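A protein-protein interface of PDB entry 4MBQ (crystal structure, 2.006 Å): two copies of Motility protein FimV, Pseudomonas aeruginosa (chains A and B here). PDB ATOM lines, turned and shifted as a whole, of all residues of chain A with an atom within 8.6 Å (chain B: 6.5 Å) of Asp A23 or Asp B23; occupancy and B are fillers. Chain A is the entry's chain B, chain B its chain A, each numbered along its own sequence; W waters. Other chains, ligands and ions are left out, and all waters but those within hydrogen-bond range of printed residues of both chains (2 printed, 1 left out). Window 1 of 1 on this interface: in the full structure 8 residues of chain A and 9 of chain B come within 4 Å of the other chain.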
ATOM      1  N   ASP A  16     -14.221   8.874  -0.377  1.00  0.00           N
ATOM      2  CA  ASP A  16     -13.388   8.377   0.709  1.00  0.00           C
ATOM      3  C   ASP A  16     -12.062   7.855   0.166  1.00  0.00           C
ATOM      4  O   ASP A  16     -11.017   8.019   0.794  1.00  0.00           O
ATOM      5  CB  ASP A  16     -14.113   7.275   1.485  1.00  0.00           C
ATOM      6  N   GLU A  17     -12.109   7.226  -1.005  1.00  0.00           N
ATOM      7  CA  GLU A  17     -10.896   6.715  -1.628  1.00  0.00           C
ATOM      8  C   GLU A  17     -10.088   7.858  -2.238  1.00  0.00           C
ATOM      9  O   GLU A  17      -8.859   7.807  -2.279  1.00  0.00           O
ATOM     10  CB  GLU A  17     -11.216   5.647  -2.682  1.00  0.00           C
ATOM     11  CG  GLU A  17     -11.889   6.170  -3.941  1.00  0.00           C
ATOM     12  N   ALA A  18     -10.786   8.892  -2.696  1.00  0.00           N
ATOM     13  CA  ALA A  18     -10.134  10.061  -3.272  1.00  0.00           C
ATOM     14  C   ALA A  18      -9.433  10.870  -2.187  1.00  0.00           C
ATOM     15  O   ALA A  18      -8.360  11.433  -2.411  1.00  0.00           O
ATOM     16  CB  ALA A  18     -11.146  10.922  -4.005  1.00  0.00           C
ATOM     17  N   ALA A  19     -10.050  10.928  -1.011  1.00  0.00           N
ATOM     18  CA  ALA A  19      -9.463  11.620   0.130  1.00  0.00           C
ATOM     19  C   ALA A  19      -8.178  10.927   0.574  1.00  0.00           C
ATOM     20  O   ALA A  19      -7.183  11.583   0.883  1.00  0.00           O
ATOM     21  CB  ALA A  19     -10.458  11.688   1.278  1.00  0.00           C
ATOM     22  N   THR A  20      -8.207   9.599   0.598  1.00  0.00           N
ATOM     23  CA  THR A  20      -7.034   8.808   0.951  1.00  0.00           C
ATOM     24  C   THR A  20      -5.915   9.018  -0.060  1.00  0.00           C
ATOM     25  O   THR A  20      -4.750   9.180   0.307  1.00  0.00           O
ATOM     26  CB  THR A  20      -7.363   7.305   1.014  1.00  0.00           C
ATOM     27  OG1 THR A  20      -8.419   7.082   1.956  1.00  0.00           O
ATOM     28  CG2 THR A  20      -6.135   6.508   1.434  1.00  0.00           C
ATOM     29  N   LYS A  21      -6.276   9.017  -1.339  1.00  0.00           N
ATOM     30  CA  LYS A  21      -5.293   9.186  -2.400  1.00  0.00           C
ATOM     31  C   LYS A  21      -4.678  10.583  -2.389  1.00  0.00           C
ATOM     32  O   LYS A  21      -3.513  10.753  -2.737  1.00  0.00           O
ATOM     33  CB  LYS A  21      -5.910   8.855  -3.764  1.00  0.00           C
ATOM     34  CG  LYS A  21      -6.167   7.363  -3.954  1.00  0.00           C
ATOM     35  CD  LYS A  21      -6.863   7.054  -5.270  1.00  0.00           C
ATOM     36  CE  LYS A  21      -7.049   5.548  -5.434  1.00  0.00           C
ATOM     37  NZ  LYS A  21      -7.780   5.196  -6.678  1.00  0.00           N
ATOM     38  N   LEU A  22      -5.460  11.575  -1.977  1.00  0.00           N
ATOM     39  CA  LEU A  22      -4.957  12.940  -1.866  1.00  0.00           C
ATOM     40  C   LEU A  22      -3.859  13.028  -0.811  1.00  0.00           C
ATOM     41  O   LEU A  22      -2.844  13.697  -1.008  1.00  0.00           O
ATOM     42  CB  LEU A  22      -6.091  13.913  -1.537  1.00  0.00           C
ATOM     43  CG  LEU A  22      -6.927  14.389  -2.728  1.00  0.00           C
ATOM     44  CD1 LEU A  22      -8.109  15.228  -2.264  1.00  0.00           C
ATOM     45  CD2 LEU A  22      -6.050  15.177  -3.683  1.00  0.00           C
ATOM     46  N   ASP A  23      -4.063  12.347   0.310  1.00  0.00           N
ATOM     47  CA  ASP A  23      -3.051  12.320   1.362  1.00  0.00           C
ATOM     48  C   ASP A  23      -1.827  11.514   0.935  1.00  0.00           C
ATOM     49  O   ASP A  23      -0.701  11.864   1.281  1.00  0.00           O
ATOM     50  CB  ASP A  23      -3.637  11.796   2.673  1.00  0.00           C
ATOM     51  CG  ASP A  23      -4.380  12.872   3.442  1.00  0.00           C
ATOM     52  OD1 ASP A  23      -3.826  13.979   3.616  1.00  0.00           O
ATOM     53  OD2 ASP A  23      -5.524  12.618   3.867  1.00  0.00           O
ATOM     54  N   LEU A  24      -2.051  10.450   0.169  1.00  0.00           N
ATOM     55  CA  LEU A  24      -0.949   9.669  -0.388  1.00  0.00           C
ATOM     56  C   LEU A  24      -0.126  10.509  -1.356  1.00  0.00           C
ATOM     57  O   LEU A  24       1.101  10.411  -1.388  1.00  0.00           O
ATOM     58  CB  LEU A  24      -1.464   8.414  -1.098  1.00  0.00           C
ATOM     59  CG  LEU A  24      -1.895   7.239  -0.223  1.00  0.00           C
ATOM     60  CD1 LEU A  24      -2.094   5.995  -1.074  1.00  0.00           C
ATOM     61  CD2 LEU A  24      -0.879   6.989   0.877  1.00  0.00           C
ATOM     62  N   ALA A  25      -0.806  11.332  -2.148  1.00  0.00           N
ATOM     63  CA  ALA A  25      -0.126  12.210  -3.089  1.00  0.00           C
ATOM     64  C   ALA A  25       0.739  13.219  -2.346  1.00  0.00           C
ATOM     65  O   ALA A  25       1.870  13.492  -2.750  1.00  0.00           O
ATOM     66  CB  ALA A  25      -1.130  12.919  -3.985  1.00  0.00           C
ATOM     67  N   ARG A  26       0.199  13.770  -1.263  1.00  0.00           N
ATOM     68  CA  ARG A  26       0.948  14.687  -0.411  1.00  0.00           C
ATOM     69  C   ARG A  26       2.180  13.996   0.163  1.00  0.00           C
ATOM     70  O   ARG A  26       3.229  14.618   0.336  1.00  0.00           O
ATOM     71  CB  ARG A  26       0.067  15.225   0.722  1.00  0.00           C
ATOM     72  CG  ARG A  26      -1.106  16.081   0.251  1.00  0.00           C
ATOM     73  CD  ARG A  26      -1.956  16.578   1.418  1.00  0.00           C
ATOM     74  NE  ARG A  26      -3.124  17.323   0.952  1.00  0.00           N
ATOM     75  CZ  ARG A  26      -4.382  16.907   1.071  1.00  0.00           C
ATOM     76  NH1 ARG A  26      -4.650  15.750   1.662  1.00  0.00           N
ATOM     77  NH2 ARG A  26      -5.376  17.655   0.609  1.00  0.00           N
ATOM     78  N   ALA A  27       2.046  12.706   0.451  1.00  0.00           N
ATOM     79  CA  ALA A  27       3.159  11.917   0.971  1.00  0.00           C
ATOM     80  C   ALA A  27       4.262  11.774  -0.074  1.00  0.00           C
ATOM     81  O   ALA A  27       5.447  11.891   0.245  1.00  0.00           O
ATOM     82  CB  ALA A  27       2.673  10.554   1.426  1.00  0.00           C
ATOM     83  N   TYR A  28       3.865  11.528  -1.321  1.00  0.00           N
ATOM     84  CA  TYR A  28       4.817  11.400  -2.423  1.00  0.00           C
ATOM     85  C   TYR A  28       5.567  12.702  -2.670  1.00  0.00           C
ATOM     86  O   TYR A  28       6.762  12.697  -2.965  1.00  0.00           O
ATOM     87  CB  TYR A  28       4.108  10.956  -3.707  1.00  0.00           C
ATOM     88  CG  TYR A  28       4.048   9.456  -3.896  1.00  0.00           C
ATOM     89  CD1 TYR A  28       5.052   8.783  -4.579  1.00  0.00           C
ATOM     90  CD2 TYR A  28       2.987   8.714  -3.397  1.00  0.00           C
ATOM     91  CE1 TYR A  28       5.003   7.412  -4.756  1.00  0.00           C
ATOM     92  CE2 TYR A  28       2.930   7.342  -3.568  1.00  0.00           C
ATOM     93  CZ  TYR A  28       3.939   6.698  -4.249  1.00  0.00           C
ATOM     94  OH  TYR A  28       3.882   5.335  -4.422  1.00  0.00           O
ATOM     95  N   ILE A  29       4.857  13.818  -2.553  1.00  0.00           N
ATOM     96  CA  ILE A  29       5.459  15.130  -2.742  1.00  0.00           C
ATOM     97  C   ILE A  29       6.513  15.392  -1.671  1.00  0.00           C
ATOM     98  O   ILE A  29       7.614  15.851  -1.968  1.00  0.00           O
ATOM     99  CB  ILE A  29       4.395  16.241  -2.718  1.00  0.00           C
ATOM    100  CG1 ILE A  29       3.429  16.069  -3.892  1.00  0.00           C
ATOM    101  CG2 ILE A  29       5.050  17.611  -2.780  1.00  0.00           C
ATOM    102  CD1 ILE A  29       2.319  17.095  -3.923  1.00  0.00           C
ATOM    103  N   ASP A  30       6.178  15.077  -0.425  1.00  0.00           N
ATOM    104  CA  ASP A  30       7.120  15.248   0.674  1.00  0.00           C
ATOM    105  C   ASP A  30       8.302  14.290   0.582  1.00  0.00           C
ATOM    106  O   ASP A  30       9.351  14.532   1.175  1.00  0.00           O
ATOM    107  CB  ASP A  30       6.410  15.130   2.022  1.00  0.00           C
ATOM    108  CG  ASP A  30       5.704  16.413   2.412  1.00  0.00           C
ATOM    109  OD1 ASP A  30       6.304  17.495   2.235  1.00  0.00           O
ATOM    110  OD2 ASP A  30       4.552  16.351   2.879  1.00  0.00           O
ATOM    111  N   MET A  31       8.132  13.209  -0.175  1.00  0.00           N
ATOM    112  CA  MET A  31       9.229  12.284  -0.437  1.00  0.00           C
ATOM    113  C   MET A  31      10.098  12.791  -1.578  1.00  0.00           C
ATOM    114  O   MET A  31      11.177  12.257  -1.833  1.00  0.00           O
ATOM    115  CB  MET A  31       8.697  10.890  -0.776  1.00  0.00           C
ATOM    116  CG  MET A  31       8.402  10.026   0.432  1.00  0.00           C
ATOM    117  SD  MET A  31       7.998   8.325  -0.010  1.00  0.00           S
ATOM    118  CE  MET A  31       6.431   8.543  -0.837  1.00  0.00           C
ATOM    119  N   ALA A  37       3.388  11.102  -7.334  1.00  0.00           N
ATOM    120  CA  ALA A  37       2.293  11.972  -6.922  1.00  0.00           C
ATOM    121  C   ALA A  37       1.341  12.258  -8.082  1.00  0.00           C
ATOM    122  O   ALA A  37       0.124  12.275  -7.904  1.00  0.00           O
ATOM    123  CB  ALA A  37       2.836  13.274  -6.341  1.00  0.00           C
ATOM    124  N   ILE A  40      -0.991   9.282  -8.890  1.00  0.00           N
ATOM    125  CA  ILE A  40      -2.049   9.195  -7.890  1.00  0.00           C
ATOM    126  C   ILE A  40      -3.090  10.294  -8.074  1.00  0.00           C
ATOM    127  O   ILE A  40      -4.292  10.048  -7.963  1.00  0.00           O
ATOM    128  CB  ILE A  40      -1.478   9.278  -6.463  1.00  0.00           C
ATOM    129  CG1 ILE A  40      -0.641   8.039  -6.154  1.00  0.00           C
ATOM    130  CG2 ILE A  40      -2.593   9.410  -5.443  1.00  0.00           C
ATOM    131  CD1 ILE A  40      -0.276   7.916  -4.692  1.00  0.00           C
ATOM    132  N   LEU A  41      -2.621  11.507  -8.352  1.00  0.00           N
ATOM    133  CA  LEU A  41      -3.512  12.647  -8.546  1.00  0.00           C
ATOM    134  C   LEU A  41      -4.383  12.497  -9.792  1.00  0.00           C
ATOM    135  O   LEU A  41      -5.497  13.021  -9.843  1.00  0.00           O
ATOM    136  CB  LEU A  41      -2.715  13.953  -8.600  1.00  0.00           C
ATOM    137  CG  LEU A  41      -2.127  14.392  -7.256  1.00  0.00           C
ATOM    138  CD1 LEU A  41      -1.153  15.549  -7.428  1.00  0.00           C
ATOM    139  CD2 LEU A  41      -3.240  14.763  -6.289  1.00  0.00           C
ATOM    140  N   VAL A  44      -7.358  10.819  -8.578  1.00  0.00           N
ATOM    141  CA  VAL A  44      -8.213  11.725  -7.815  1.00  0.00           C
ATOM    142  C   VAL A  44      -9.095  12.566  -8.746  1.00  0.00           C
ATOM    143  O   VAL A  44     -10.285  12.762  -8.484  1.00  0.00           O
ATOM    144  CB  VAL A  44      -7.382  12.647  -6.897  1.00  0.00           C
ATOM    145  CG1 VAL A  44      -8.281  13.645  -6.183  1.00  0.00           C
ATOM    146  CG2 VAL A  44      -6.597  11.820  -5.894  1.00  0.00           C
ATOM    147  N   GLU A  55      -8.461  20.337  -5.342  1.00  0.00           N
ATOM    148  CA  GLU A  55      -7.216  20.167  -4.604  1.00  0.00           C
ATOM    149  C   GLU A  55      -6.158  19.454  -5.437  1.00  0.00           C
ATOM    150  O   GLU A  55      -4.976  19.802  -5.388  1.00  0.00           O
ATOM    151  CB  GLU A  55      -7.460  19.408  -3.296  1.00  0.00           C
ATOM    152  CG  GLU A  55      -6.193  18.938  -2.581  1.00  0.00           C
ATOM    153  CD  GLU A  55      -5.402  20.066  -1.925  1.00  0.00           C
ATOM    154  OE1 GLU A  55      -5.642  21.251  -2.243  1.00  0.00           O
ATOM    155  OE2 GLU A  55      -4.535  19.763  -1.079  1.00  0.00           O
ATOM    156  N   LEU A  59      -2.546  20.900  -6.421  1.00  0.00           N
ATOM    157  CA  LEU A  59      -1.313  20.163  -6.161  1.00  0.00           C
ATOM    158  C   LEU A  59      -0.501  19.953  -7.437  1.00  0.00           C
ATOM    159  O   LEU A  59       0.723  20.101  -7.433  1.00  0.00           O
ATOM    160  CB  LEU A  59      -1.616  18.819  -5.497  1.00  0.00           C
ATOM    161  CG  LEU A  59      -2.058  18.904  -4.036  1.00  0.00           C
ATOM    162  CD1 LEU A  59      -2.373  17.524  -3.474  1.00  0.00           C
ATOM    163  CD2 LEU A  59      -0.988  19.596  -3.202  1.00  0.00           C
ATOM    164  N   ALA B  18       9.694  12.561   8.393  1.00  0.00           N
ATOM    165  CA  ALA B  18       8.654  12.839   9.376  1.00  0.00           C
ATOM    166  C   ALA B  18       7.426  13.474   8.721  1.00  0.00           C
ATOM    167  O   ALA B  18       6.290  13.107   9.023  1.00  0.00           O
ATOM    168  CB  ALA B  18       9.193  13.738  10.475  1.00  0.00           C
ATOM    169  N   ALA B  19       7.663  14.426   7.822  1.00  0.00           N
ATOM    170  CA  ALA B  19       6.576  15.111   7.127  1.00  0.00           C
ATOM    171  C   ALA B  19       5.808  14.150   6.224  1.00  0.00           C
ATOM    172  O   ALA B  19       4.597  14.283   6.047  1.00  0.00           O
ATOM    173  CB  ALA B  19       7.112  16.285   6.323  1.00  0.00           C
ATOM    174  N   THR B  20       6.519  13.185   5.651  1.00  0.00           N
ATOM    175  CA  THR B  20       5.891  12.170   4.815  1.00  0.00           C
ATOM    176  C   THR B  20       5.003  11.259   5.654  1.00  0.00           C
ATOM    177  O   THR B  20       3.885  10.927   5.259  1.00  0.00           O
ATOM    178  CB  THR B  20       6.938  11.307   4.092  1.00  0.00           C
ATOM    179  OG1 THR B  20       7.730  12.134   3.230  1.00  0.00           O
ATOM    180  CG2 THR B  20       6.251  10.231   3.261  1.00  0.00           C
ATOM    181  N   LYS B  21       5.508  10.864   6.819  1.00  0.00           N
ATOM    182  CA  LYS B  21       4.770   9.981   7.714  1.00  0.00           C
ATOM    183  C   LYS B  21       3.507  10.645   8.252  1.00  0.00           C
ATOM    184  O   LYS B  21       2.492   9.979   8.455  1.00  0.00           O
ATOM    185  CB  LYS B  21       5.660   9.508   8.868  1.00  0.00           C
ATOM    186  CG  LYS B  21       6.733   8.506   8.458  1.00  0.00           C
ATOM    187  CD  LYS B  21       7.494   8.008   9.674  1.00  0.00           C
ATOM    188  CE  LYS B  21       8.481   6.908   9.317  1.00  0.00           C
ATOM    189  NZ  LYS B  21       9.615   7.423   8.504  1.00  0.00           N
ATOM    190  N   LEU B  22       3.572  11.953   8.489  1.00  0.00           N
ATOM    191  CA  LEU B  22       2.391  12.711   8.892  1.00  0.00           C
ATOM    192  C   LEU B  22       1.277  12.564   7.853  1.00  0.00           C
ATOM    193  O   LEU B  22       0.121  12.329   8.202  1.00  0.00           O
ATOM    194  CB  LEU B  22       2.731  14.191   9.111  1.00  0.00           C
ATOM    195  CG  LEU B  22       3.411  14.554  10.439  1.00  0.00           C
ATOM    196  CD1 LEU B  22       3.867  16.006  10.438  1.00  0.00           C
ATOM    197  CD2 LEU B  22       2.479  14.291  11.611  1.00  0.00           C
ATOM    198  N   ASP B  23       1.634  12.691   6.579  1.00  0.00           N
ATOM    199  CA  ASP B  23       0.665  12.538   5.494  1.00  0.00           C
ATOM    200  C   ASP B  23       0.145  11.110   5.415  1.00  0.00           C
ATOM    201  O   ASP B  23      -1.049  10.885   5.221  1.00  0.00           O
ATOM    202  CB  ASP B  23       1.287  12.916   4.154  1.00  0.00           C
ATOM    203  CG  ASP B  23       1.660  14.373   4.074  1.00  0.00           C
ATOM    204  OD1 ASP B  23       0.841  15.236   4.457  1.00  0.00           O
ATOM    205  OD2 ASP B  23       2.784  14.651   3.621  1.00  0.00           O
ATOM    206  N   LEU B  24       1.052  10.147   5.557  1.00  0.00           N
ATOM    207  CA  LEU B  24       0.676   8.743   5.544  1.00  0.00           C
ATOM    208  C   LEU B  24      -0.278   8.442   6.691  1.00  0.00           C
ATOM    209  O   LEU B  24      -1.255   7.718   6.519  1.00  0.00           O
ATOM    210  CB  LEU B  24       1.915   7.846   5.621  1.00  0.00           C
ATOM    211  CG  LEU B  24       2.782   7.817   4.361  1.00  0.00           C
ATOM    212  CD1 LEU B  24       3.954   6.866   4.528  1.00  0.00           C
ATOM    213  CD2 LEU B  24       1.944   7.418   3.156  1.00  0.00           C
ATOM    214  N   ALA B  25       0.004   9.011   7.860  1.00  0.00           N
ATOM    215  CA  ALA B  25      -0.877   8.860   9.012  1.00  0.00           C
ATOM    216  C   ALA B  25      -2.277   9.391   8.703  1.00  0.00           C
ATOM    217  O   ALA B  25      -3.277   8.781   9.080  1.00  0.00           O
ATOM    218  CB  ALA B  25      -0.290   9.559  10.232  1.00  0.00           C
ATOM    219  N   ARG B  26      -2.343  10.522   8.006  1.00  0.00           N
ATOM    220  CA  ARG B  26      -3.622  11.091   7.596  1.00  0.00           C
ATOM    221  C   ARG B  26      -4.338  10.175   6.607  1.00  0.00           C
ATOM    222  O   ARG B  26      -5.566  10.089   6.604  1.00  0.00           O
ATOM    223  CB  ARG B  26      -3.427  12.480   6.984  1.00  0.00           C
ATOM    224  CG  ARG B  26      -2.884  13.512   7.957  1.00  0.00           C
ATOM    225  CD  ARG B  26      -2.820  14.890   7.321  1.00  0.00           C
ATOM    226  NE  ARG B  26      -2.273  15.889   8.233  1.00  0.00           N
ATOM    227  CZ  ARG B  26      -1.006  16.292   8.230  1.00  0.00           C
ATOM    228  NH1 ARG B  26      -0.148  15.784   7.356  1.00  0.00           N
ATOM    229  NH2 ARG B  26      -0.598  17.208   9.099  1.00  0.00           N
ATOM    230  N   ALA B  27      -3.560   9.491   5.772  1.00  0.00           N
ATOM    231  CA  ALA B  27      -4.110   8.531   4.822  1.00  0.00           C
ATOM    232  C   ALA B  27      -4.719   7.328   5.539  1.00  0.00           C
ATOM    233  O   ALA B  27      -5.778   6.837   5.146  1.00  0.00           O
ATOM    234  CB  ALA B  27      -3.040   8.082   3.832  1.00  0.00           C
ATOM    235  N   TYR B  28      -4.044   6.857   6.586  1.00  0.00           N
ATOM    236  CA  TYR B  28      -4.547   5.752   7.398  1.00  0.00           C
ATOM    237  C   TYR B  28      -5.828   6.157   8.116  1.00  0.00           C
ATOM    238  O   TYR B  28      -6.773   5.373   8.211  1.00  0.00           O
ATOM    239  CB  TYR B  28      -3.503   5.310   8.426  1.00  0.00           C
ATOM    240  CG  TYR B  28      -2.452   4.357   7.901  1.00  0.00           C
ATOM    241  CD1 TYR B  28      -2.369   3.056   8.378  1.00  0.00           C
ATOM    242  CD2 TYR B  28      -1.541   4.758   6.934  1.00  0.00           C
ATOM    243  CE1 TYR B  28      -1.408   2.181   7.907  1.00  0.00           C
ATOM    244  CE2 TYR B  28      -0.580   3.891   6.454  1.00  0.00           C
ATOM    245  CZ  TYR B  28      -0.514   2.607   6.948  1.00  0.00           C
ATOM    246  OH  TYR B  28       0.444   1.744   6.473  1.00  0.00           O
ATOM    247  N   ASP B  30      -7.946   8.309   7.070  1.00  0.00           N
ATOM    248  CA  ASP B  30      -8.985   8.306   6.039  1.00  0.00           C
ATOM    249  C   ASP B  30      -9.609   6.926   5.879  1.00  0.00           C
ATOM    250  O   ASP B  30     -10.814   6.799   5.669  1.00  0.00           O
ATOM    251  CB  ASP B  30      -8.411   8.722   4.686  1.00  0.00           C
ATOM    252  CG  ASP B  30      -7.968  10.163   4.653  1.00  0.00           C
ATOM    253  OD1 ASP B  30      -8.577  11.002   5.350  1.00  0.00           O
ATOM    254  OD2 ASP B  30      -7.007  10.453   3.912  1.00  0.00           O
HETATM  255  O   HOH W   1      -7.689  13.960   4.605  1.00  0.00           O
HETATM  256  O   HOH W   2       1.637  17.982   3.609  1.00  0.00           O
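Of chain B, only Asp B23 (3.6 Å), Arg B26 (3.7 Å), Ala B27 (3.9 Å) and Asp B30 (2.6 Å) come within 4 Å of Asp A23. Printed residues of chain A within 4 Å of Asp B23: Asp A23, Arg A26, Ala A27 and Asp A30. Of the printed residues of chain A, Asp B30 touches Ala A19 (3.2 Å), Thr A20 (3.2 Å) and Asp A23 (2.6 Å). Printed residues of chain A within 4 Å of Arg B26: Asp A23. Printed residues of chain A within 4 Å of Thr B20: Ala A27 (3.5 Å), Asp A30 (3.5 Å) and Met A31 (3.6 Å). Of the printed residues of chain B, Thr A20 touches Ala B27 (3.7 Å) and Asp B30 (3.2 Å). Ile A40 touches none of the printed residues of chain B. Ala A37 touches none of the printed residues of chain B. The nearest residue of chain B that does not touch Asp A23 is Leu B24 (4.9 Å). The nearest printed residue of chain B that does not touch Ala A27 is Ala B19 (5.8 Å).
Printed residues of chain B that touch a printed residue of chain A: Ala B19, Thr B20, Asp B23, Leu B24, Arg B26, Ala B27 and Asp B30. Hydrophobic or aromatic side chains of chain B within 4 Å of the printed part of chain A: Leu B24 and Ala B27. Hydrophobic or aromatic side chains of chain A within 4 Å of the printed part of chain B: Leu A24, Ala A27 and Met A31. Among the printed residues, 17 pairs touch across the chains.
Ala A19 touches Asp B30, and with the chains exchanged Asp A30 touches Ala B19. Asp A23 touches Ala B27, and with the chains exchanged Ala A27 touches Asp B23. Leu A24 touches its own counterpart, Leu B24. Leu A24 touches Ala B27, and with the chains exchanged Ala A27 touches Leu B24. 12 positions are printed for both chains. Of the 17 pairs that touch across the chains among the printed residues, 16 have their exchanged pair printed and touching as well.
Water W1 bridges the side-chain carboxylate of Asp A23 (2.7 Å) and the side-chain carboxylate of Asp B30 (3.2 Å). Water W2 bridges the side-chain carboxylate (OD1) of Asp B23 (3.0 Å) and the side-chain carboxylate (OD2) of Asp A30 (3.4 Å).
OE2 of Glu A55 is in salt-bridge range of NH2 of Arg A26 (2.8 Å). The backbone carbonyl oxygen of Asp A16 lies within hydrogen-bond range of the side-chain hydroxyl of Thr A20, 3.0 Å away. The side-chain carboxylate (OD1) of Asp A23 lies within salt-bridge range of the guanidinium group (NH1) of Arg A26 (2.8 Å). The side-chain carboxylate (OD1) of Asp B23 is in salt-bridge range of the guanidinium group (NH1) of Arg B26, 3.1 Å away.
Thr A20 touches Ala B27. CG of Asp A23 touches CB of Arg B26, 3.7 Å away. N of Ala B27 touches CB of Asp A23, 3.9 Å away. Leu A24 touches Leu B24 (CD2 to CD2, 3.7 Å). CB of Ala B27 touches CD2 of Leu A24, at 3.8 Å. O of Ala A27 touches CG2 of Thr B20, at 3.5 Å. Ala A27 touches Asp B23. Ala A27 touches Leu B24 (CB to CD2, 3.7 Å). OD2 of Asp A30 touches O of Ala B19, at 3.8 Å. CG of Met A31 touches CG2 of Thr B20 (3.6 Å).
The side-chain carboxylate (OD2) of Asp A23 sits close to the side-chain carboxylate (OD2) of Asp B30. The side-chain carboxylate (OD2) of Asp B23 sits close to the backbone carbonyl oxygen (O) of Arg A26. The side-chain carboxylate (OD2) of Asp B23 sits close to the side-chain carboxylate (OD2) of Asp A30. The side-chain carboxylate (OD2) of Asp B30 lies close to the backbone carbonyl oxygen (O) of Ala A19 (3.2 Å).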
